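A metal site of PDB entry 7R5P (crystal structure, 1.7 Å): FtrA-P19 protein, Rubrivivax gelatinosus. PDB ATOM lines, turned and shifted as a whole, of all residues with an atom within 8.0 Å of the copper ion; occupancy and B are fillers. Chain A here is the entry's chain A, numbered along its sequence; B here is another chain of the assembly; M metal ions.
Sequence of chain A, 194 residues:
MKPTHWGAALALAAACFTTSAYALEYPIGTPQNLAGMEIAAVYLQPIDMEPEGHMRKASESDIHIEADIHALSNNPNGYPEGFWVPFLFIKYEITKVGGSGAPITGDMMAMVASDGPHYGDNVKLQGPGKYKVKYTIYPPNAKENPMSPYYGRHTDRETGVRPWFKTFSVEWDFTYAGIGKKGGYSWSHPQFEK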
ATOM      1  N   LEU A  44       1.864   7.076   6.581  1.00  0.00           N
ATOM      2  CA  LEU A  44       0.595   6.793   5.918  1.00  0.00           C
ATOM      3  C   LEU A  44       0.430   7.846   4.840  1.00  0.00           C
ATOM      4  O   LEU A  44       1.394   8.599   4.569  1.00  0.00           O
ATOM      5  CB  LEU A  44      -0.602   6.799   6.873  1.00  0.00           C
ATOM      6  CG  LEU A  44      -0.839   8.100   7.687  1.00  0.00           C
ATOM      7  CD1 LEU A  44      -2.310   8.295   7.954  1.00  0.00           C
ATOM      8  CD2 LEU A  44      -0.098   8.078   8.982  1.00  0.00           C
ATOM      9  N   GLN A  45      -0.715   7.825   4.161  1.00  0.00           N
ATOM     10  CA  GLN A  45      -0.988   8.752   3.076  1.00  0.00           C
ATOM     11  C   GLN A  45      -0.936  10.217   3.571  1.00  0.00           C
ATOM     12  O   GLN A  45      -1.256  10.443   4.749  1.00  0.00           O
ATOM     13  CB  GLN A  45      -2.344   8.438   2.398  1.00  0.00           C
ATOM     14  CG  GLN A  45      -3.601   8.652   3.259  1.00  0.00           C
ATOM     15  CD  GLN A  45      -3.900   7.586   4.297  1.00  0.00           C
ATOM     16  OE1 GLN A  45      -3.205   6.570   4.434  1.00  0.00           O
ATOM     17  NE2 GLN A  45      -4.959   7.805   5.045  1.00  0.00           N
ATOM     18  N   ILE A  47      -2.122  13.841   4.658  1.00  0.00           N
ATOM     19  CA  ILE A  47      -3.402  14.209   5.264  1.00  0.00           C
ATOM     20  C   ILE A  47      -3.714  15.704   5.097  1.00  0.00           C
ATOM     21  O   ILE A  47      -2.866  16.467   4.628  1.00  0.00           O
ATOM     22  CB  ILE A  47      -3.415  13.765   6.761  1.00  0.00           C
ATOM     23  CG1 ILE A  47      -2.297  14.443   7.575  1.00  0.00           C
ATOM     24  CG2 ILE A  47      -3.351  12.235   6.902  1.00  0.00           C
ATOM     25  CD1 ILE A  47      -2.644  15.838   8.224  1.00  0.00           C
ATOM     26  N   ASP A  48      -4.929  16.085   5.533  1.00  0.00           N
ATOM     27  CA  ASP A  48      -5.455  17.458   5.613  1.00  0.00           C
ATOM     28  C   ASP A  48      -5.567  17.758   7.098  1.00  0.00           C
ATOM     29  O   ASP A  48      -5.982  16.891   7.868  1.00  0.00           O
ATOM     30  CB  ASP A  48      -6.844  17.536   4.962  1.00  0.00           C
ATOM     31  CG  ASP A  48      -6.860  17.238   3.471  1.00  0.00           C
ATOM     32  OD1 ASP A  48      -5.777  17.308   2.843  1.00  0.00           O
ATOM     33  OD2 ASP A  48      -7.955  16.919   2.951  1.00  0.00           O
ATOM     34  N   MET A  49      -5.203  18.983   7.510  1.00  0.00           N
ATOM     35  CA  MET A  49      -5.200  19.355   8.917  1.00  0.00           C
ATOM     36  C   MET A  49      -5.708  20.781   9.142  1.00  0.00           C
ATOM     37  O   MET A  49      -5.492  21.651   8.285  1.00  0.00           O
ATOM     38  CB  MET A  49      -3.742  19.257   9.437  1.00  0.00           C
ATOM     39  CG  MET A  49      -3.630  19.254  10.942  1.00  0.00           C
ATOM     40  SD  MET A  49      -1.982  19.750  11.512  1.00  0.00           S
ATOM     41  CE  MET A  49      -2.029  21.490  11.150  1.00  0.00           C
ATOM     42  N   MET A  55       0.788  22.324   7.505  1.00  0.00           N
ATOM     43  CA  MET A  55       1.252  21.156   6.764  1.00  0.00           C
ATOM     44  C   MET A  55       1.535  21.544   5.326  1.00  0.00           C
ATOM     45  O   MET A  55       0.798  22.353   4.753  1.00  0.00           O
ATOM     46  CB  MET A  55       0.140  20.073   6.744  1.00  0.00           C
ATOM     47  CG  MET A  55      -0.149  19.436   8.076  1.00  0.00           C
ATOM     48  SD  MET A  55       1.212  18.392   8.631  1.00  0.00           S
ATOM     49  CE  MET A  55       1.940  19.468   9.992  1.00  0.00           C
ATOM     50  N   HIS A  64       2.632  11.040   5.165  1.00  0.00           N
ATOM     51  CA  HIS A  64       2.431  11.761   6.423  1.00  0.00           C
ATOM     52  C   HIS A  64       3.288  10.947   7.345  1.00  0.00           C
ATOM     53  O   HIS A  64       2.972   9.783   7.563  1.00  0.00           O
ATOM     54  CB  HIS A  64       0.967  11.774   6.882  1.00  0.00           C
ATOM     55  CG  HIS A  64       0.758  12.652   8.102  1.00  0.00           C
ATOM     56  ND1 HIS A  64       1.019  14.025   8.056  1.00  0.00           N
ATOM     57  CD2 HIS A  64       0.299  12.352   9.345  1.00  0.00           C
ATOM     58  CE1 HIS A  64       0.711  14.499   9.261  1.00  0.00           C
ATOM     59  NE2 HIS A  64       0.306  13.523  10.069  1.00  0.00           N
ATOM     60  N   ILE A  65       4.388  11.502   7.839  1.00  0.00           N
ATOM     61  CA  ILE A  65       5.262  10.755   8.744  1.00  0.00           C
ATOM     62  C   ILE A  65       4.830  11.046  10.162  1.00  0.00           C
ATOM     63  O   ILE A  65       4.397  12.170  10.442  1.00  0.00           O
ATOM     64  CB  ILE A  65       6.771  11.016   8.484  1.00  0.00           C
ATOM     65  CG1 ILE A  65       7.645   9.993   9.223  1.00  0.00           C
ATOM     66  CG2 ILE A  65       7.218  12.467   8.836  1.00  0.00           C
ATOM     67  CD1 ILE A  65       8.920   9.633   8.553  1.00  0.00           C
ATOM     68  N   GLU A  66       4.914  10.038  11.043  1.00  0.00           N
ATOM     69  CA  GLU A  66       4.485  10.174  12.397  1.00  0.00           C
ATOM     70  C   GLU A  66       5.434   9.604  13.392  1.00  0.00           C
ATOM     71  O   GLU A  66       6.050   8.582  13.146  1.00  0.00           O
ATOM     72  CB  GLU A  66       3.103   9.488  12.608  1.00  0.00           C
ATOM     73  CG  GLU A  66       1.946  10.127  11.864  1.00  0.00           C
ATOM     74  CD  GLU A  66       0.581   9.505  12.128  1.00  0.00           C
ATOM     75  OE1 GLU A  66       0.522   8.460  12.808  1.00  0.00           O
ATOM     76  OE2 GLU A  66      -0.430  10.092  11.660  1.00  0.00           O
ATOM     77  N   ALA A  67       5.422  10.223  14.600  1.00  0.00           N
ATOM     78  CA  ALA A  67       6.132   9.704  15.768  1.00  0.00           C
ATOM     79  C   ALA A  67       5.031   9.381  16.769  1.00  0.00           C
ATOM     80  O   ALA A  67       4.244  10.277  17.129  1.00  0.00           O
ATOM     81  CB  ALA A  67       7.072  10.773  16.340  1.00  0.00           C
ATOM     82  N   MET A 109       4.482  18.340  14.030  1.00  0.00           N
ATOM     83  CA  MET A 109       3.550  19.153  14.771  1.00  0.00           C
ATOM     84  C   MET A 109       2.642  18.214  15.547  1.00  0.00           C
ATOM     85  O   MET A 109       2.268  17.155  15.019  1.00  0.00           O
ATOM     86  CB  MET A 109       2.757  20.000  13.788  1.00  0.00           C
ATOM     87  CG  MET A 109       1.714  20.830  14.454  1.00  0.00           C
ATOM     88  SD  MET A 109       1.011  21.899  13.224  1.00  0.00           S
ATOM     89  CE  MET A 109      -0.100  22.871  14.304  1.00  0.00           C
ATOM     90  N   ALA A 110       2.281  18.593  16.792  1.00  0.00           N
ATOM     91  CA  ALA A 110       1.367  17.790  17.600  1.00  0.00           C
ATOM     92  C   ALA A 110      -0.016  17.951  16.982  1.00  0.00           C
ATOM     93  O   ALA A 110      -0.345  19.039  16.486  1.00  0.00           O
ATOM     94  CB  ALA A 110       1.362  18.315  19.040  1.00  0.00           C
ATOM     95  N   MET A 111      -0.777  16.870  16.916  1.00  0.00           N
ATOM     96  CA  MET A 111      -2.121  16.908  16.309  1.00  0.00           C
ATOM     97  C   MET A 111      -2.915  15.666  16.670  1.00  0.00           C
ATOM     98  O   MET A 111      -2.356  14.708  17.173  1.00  0.00           O
ATOM     99  CB  MET A 111      -2.036  17.060  14.788  1.00  0.00           C
ATOM    100  CG  MET A 111      -1.367  15.860  14.087  1.00  0.00           C
ATOM    101  SD  MET A 111      -1.114  16.124  12.335  1.00  0.00           S
ATOM    102  CE  MET A 111       0.416  16.993  12.331  1.00  0.00           C
ATOM    103  N   VAL A 112      -4.211  15.682  16.388  1.00  0.00           N
ATOM    104  CA  VAL A 112      -5.097  14.545  16.630  1.00  0.00           C
ATOM    105  C   VAL A 112      -5.704  14.002  15.326  1.00  0.00           C
ATOM    106  O   VAL A 112      -5.993  14.785  14.406  1.00  0.00           O
ATOM    107  CB  VAL A 112      -6.196  14.860  17.703  1.00  0.00           C
ATOM    108  CG1 VAL A 112      -7.336  15.682  17.129  1.00  0.00           C
ATOM    109  CG2 VAL A 112      -6.715  13.573  18.355  1.00  0.00           C
ATOM    110  N   ALA A 113      -5.854  12.665  15.260  1.00  0.00           N
ATOM    111  CA  ALA A 113      -6.504  11.939  14.141  1.00  0.00           C
ATOM    112  C   ALA A 113      -7.453  10.897  14.763  1.00  0.00           C
ATOM    113  O   ALA A 113      -7.513  10.794  15.992  1.00  0.00           O
ATOM    114  CB  ALA A 113      -5.456  11.248  13.264  1.00  0.00           C
ATOM    115  N   ASP A 115      -7.132   7.806  15.199  1.00  0.00           N
ATOM    116  CA  ASP A 115      -6.393   6.862  16.055  1.00  0.00           C
ATOM    117  C   ASP A 115      -5.777   7.547  17.301  1.00  0.00           C
ATOM    118  O   ASP A 115      -5.020   6.907  18.013  1.00  0.00           O
ATOM    119  CB  ASP A 115      -5.308   6.096  15.266  1.00  0.00           C
ATOM    120  CG  ASP A 115      -4.197   6.975  14.699  1.00  0.00           C
ATOM    121  OD1 ASP A 115      -4.470   8.160  14.373  1.00  0.00           O
ATOM    122  OD2 ASP A 115      -3.049   6.468  14.547  1.00  0.00           O
ATOM    123  N   GLY A 116      -6.084   8.841  17.517  1.00  0.00           N
ATOM    124  CA  GLY A 116      -5.605   9.576  18.689  1.00  0.00           C
ATOM    125  C   GLY A 116      -4.549  10.631  18.412  1.00  0.00           C
ATOM    126  O   GLY A 116      -4.184  10.864  17.257  1.00  0.00           O
ATOM    127  N   PRO A 117      -4.044  11.276  19.481  1.00  0.00           N
ATOM    128  CA  PRO A 117      -3.025  12.307  19.290  1.00  0.00           C
ATOM    129  C   PRO A 117      -1.662  11.742  18.925  1.00  0.00           C
ATOM    130  O   PRO A 117      -1.298  10.638  19.373  1.00  0.00           O
ATOM    131  CB  PRO A 117      -2.995  13.031  20.639  1.00  0.00           C
ATOM    132  CG  PRO A 117      -3.398  11.958  21.663  1.00  0.00           C
ATOM    133  CD  PRO A 117      -4.396  11.102  20.911  1.00  0.00           C
ATOM    134  N   HIS A 118      -0.907  12.511  18.152  1.00  0.00           N
ATOM    135  CA  HIS A 118       0.445  12.093  17.683  1.00  0.00           C
ATOM    136  C   HIS A 118       1.218  13.306  17.230  1.00  0.00           C
ATOM    137  O   HIS A 118       0.706  14.424  17.306  1.00  0.00           O
ATOM    138  CB  HIS A 118       0.334  11.043  16.490  1.00  0.00           C
ATOM    139  CG  HIS A 118      -0.369  11.638  15.319  1.00  0.00           C
ATOM    140  ND1 HIS A 118      -1.766  11.735  15.287  1.00  0.00           N
ATOM    141  CD2 HIS A 118       0.132  12.247  14.222  1.00  0.00           C
ATOM    142  CE1 HIS A 118      -2.042  12.334  14.122  1.00  0.00           C
ATOM    143  NE2 HIS A 118      -0.935  12.654  13.458  1.00  0.00           N
ATOM    144  N   TYR A 119       2.441  13.084  16.737  1.00  0.00           N
ATOM    145  CA  TYR A 119       3.288  14.119  16.146  1.00  0.00           C
ATOM    146  C   TYR A 119       3.429  13.698  14.706  1.00  0.00           C
ATOM    147  O   TYR A 119       3.705  12.525  14.445  1.00  0.00           O
ATOM    148  CB  TYR A 119       4.673  14.188  16.837  1.00  0.00           C
ATOM    149  CG  TYR A 119       4.563  14.489  18.308  1.00  0.00           C
ATOM    150  CD1 TYR A 119       4.413  15.794  18.766  1.00  0.00           C
ATOM    151  CD2 TYR A 119       4.570  13.465  19.256  1.00  0.00           C
ATOM    152  CE1 TYR A 119       4.240  16.079  20.119  1.00  0.00           C
ATOM    153  CE2 TYR A 119       4.412  13.743  20.625  1.00  0.00           C
ATOM    154  CZ  TYR A 119       4.242  15.052  21.038  1.00  0.00           C
ATOM    155  OH  TYR A 119       4.063  15.352  22.364  1.00  0.00           O
ATOM    156  N   GLY A 120       3.161  14.595  13.768  1.00  0.00           N
ATOM    157  CA  GLY A 120       3.226  14.212  12.375  1.00  0.00           C
ATOM    158  C   GLY A 120       3.607  15.352  11.457  1.00  0.00           C
ATOM    159  O   GLY A 120       3.689  16.504  11.900  1.00  0.00           O
ATOM    160  N   ASP A 121       3.907  15.026  10.192  1.00  0.00           N
ATOM    161  CA  ASP A 121       4.206  16.045   9.199  1.00  0.00           C
ATOM    162  C   ASP A 121       4.039  15.440   7.828  1.00  0.00           C
ATOM    163  O   ASP A 121       4.412  14.283   7.652  1.00  0.00           O
ATOM    164  CB  ASP A 121       5.665  16.552   9.311  1.00  0.00           C
ATOM    165  CG  ASP A 121       5.868  17.911   8.639  1.00  0.00           C
ATOM    166  OD1 ASP A 121       4.899  18.696   8.583  1.00  0.00           O
ATOM    167  OD2 ASP A 121       6.989  18.195   8.216  1.00  0.00           O
ATOM    168  N   ASN A 122       3.518  16.227   6.854  1.00  0.00           N
ATOM    169  CA  ASN A 122       3.436  15.813   5.433  1.00  0.00           C
ATOM    170  C   ASN A 122       4.818  16.038   4.817  1.00  0.00           C
ATOM    171  O   ASN A 122       5.394  17.126   4.955  1.00  0.00           O
ATOM    172  CB  ASN A 122       2.366  16.626   4.680  1.00  0.00           C
ATOM    173  CG  ASN A 122       0.948  16.119   4.845  1.00  0.00           C
ATOM    174  OD1 ASN A 122       0.713  15.052   5.416  1.00  0.00           O
ATOM    175  ND2 ASN A 122      -0.025  16.852   4.336  1.00  0.00           N
ATOM    176  N   GLY B 152      -2.973  20.595  15.970  1.00  0.00           N
ATOM    177  CA  GLY B 152      -3.855  20.404  14.839  1.00  0.00           C
ATOM    178  C   GLY B 152      -4.885  19.294  15.004  1.00  0.00           C
ATOM    179  O   GLY B 152      -4.887  18.546  15.974  1.00  0.00           O
ATOM    180  N   ARG B 153      -5.700  19.166  13.989  1.00  0.00           N
ATOM    181  CA  ARG B 153      -6.743  18.166  13.895  1.00  0.00           C
ATOM    182  C   ARG B 153      -6.822  17.685  12.451  1.00  0.00           C
ATOM    183  O   ARG B 153      -7.030  18.536  11.571  1.00  0.00           O
ATOM    184  CB  ARG B 153      -8.055  18.865  14.319  1.00  0.00           C
ATOM    185  CG  ARG B 153      -9.258  17.966  14.378  1.00  0.00           C
ATOM    186  CD  ARG B 153     -10.535  18.722  14.735  1.00  0.00           C
ATOM    187  NE  ARG B 153     -10.815  19.805  13.792  1.00  0.00           N
ATOM    188  CZ  ARG B 153     -11.568  19.702  12.694  1.00  0.00           C
ATOM    189  NH1 ARG B 153     -12.125  18.539  12.383  1.00  0.00           N
ATOM    190  NH2 ARG B 153     -11.757  20.750  11.922  1.00  0.00           N
ATOM    191  N   HIS B 154      -6.681  16.339  12.180  1.00  0.00           N
ATOM    192  CA  HIS B 154      -6.837  15.804  10.813  1.00  0.00           C
ATOM    193  C   HIS B 154      -8.298  16.064  10.394  1.00  0.00           C
ATOM    194  O   HIS B 154      -9.200  15.901  11.209  1.00  0.00           O
ATOM    195  CB  HIS B 154      -6.549  14.275  10.736  1.00  0.00           C
ATOM    196  CG  HIS B 154      -5.099  13.860  10.860  1.00  0.00           C
ATOM    197  ND1 HIS B 154      -4.660  12.671  10.365  1.00  0.00           N
ATOM    198  CD2 HIS B 154      -4.053  14.483  11.494  1.00  0.00           C
ATOM    199  CE1 HIS B 154      -3.364  12.602  10.654  1.00  0.00           C
ATOM    200  NE2 HIS B 154      -2.939  13.676  11.305  1.00  0.00           N
ATOM    201  N   ASP B 156      -9.268  15.083   6.864  1.00  0.00           N
ATOM    202  CA  ASP B 156      -9.493  14.211   5.696  1.00  0.00           C
ATOM    203  C   ASP B 156     -10.469  13.081   6.037  1.00  0.00           C
ATOM    204  O   ASP B 156     -10.626  12.739   7.201  1.00  0.00           O
ATOM    205  CB  ASP B 156      -8.152  13.654   5.172  1.00  0.00           C
ATOM    206  CG  ASP B 156      -7.353  13.002   6.268  1.00  0.00           C
ATOM    207  OD1 ASP B 156      -6.662  13.733   6.997  1.00  0.00           O
ATOM    208  OD2 ASP B 156      -7.431  11.763   6.410  1.00  0.00           O
ATOM    209  N   THR B 159      -8.748   9.687   7.986  1.00  0.00           N
ATOM    210  CA  THR B 159      -8.174   9.758   9.324  1.00  0.00           C
ATOM    211  C   THR B 159      -8.715  10.934  10.158  1.00  0.00           C
ATOM    212  O   THR B 159      -8.273  11.155  11.294  1.00  0.00           O
ATOM    213  CB  THR B 159      -6.615   9.835   9.232  1.00  0.00           C
ATOM    214  OG1 THR B 159      -6.238  11.105   8.712  1.00  0.00           O
ATOM    215  CG2 THR B 159      -5.990   8.725   8.359  1.00  0.00           C
HETATM  216 CU    CU M   1      -0.906  13.828  11.816  1.00  0.00          CU
HETATM  217 MG    MG M   2      -1.334   7.343  13.603  1.00  0.00          MG
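Merely in contact with the copper ion: Glu 66.
Of the 28 residues printed, 5 come within 4 Å of the copper ion.
A ring nitrogen (NE2) of His 118 is bound to the copper ion, at 2.0 Å.
A ring nitrogen (NE2) of His 154 of chain B is bound to the copper ion (2.1 Å).
The copper ion is bound by NE2 of His 64 (2.1 Å).
SD of Met 111 binds the copper ion (2.4 Å).
The side-chain amide oxygen (OD1) of Asn 122 sits at hydrogen-bond distance from a ring nitrogen (ND1) of His 64, 2.8 Å away.
ND1 of His 154 of chain B lies within hydrogen-bond range of OG1 of Thr 159 of chain B.
The backbone NH (N) of His 64 lies within hydrogen-bond range of the backbone carbonyl oxygen (O) of Leu 44 (2.8 Å).
A ring nitrogen (NE2) of His 118 sits close to the side-chain carboxylate (OE2) of Glu 66 (3.2 Å).
O of Asp 121 sits close to ND1 of His 64, at 3.4 Å.
O of Val 112 is in hydrogen-bond range of N of His 154 of chain B, at 2.8 Å.
A ring nitrogen (ND1) of His 118 lies within hydrogen-bond range of the backbone carbonyl oxygen (O) of Gly 116, at 3.2 Å.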
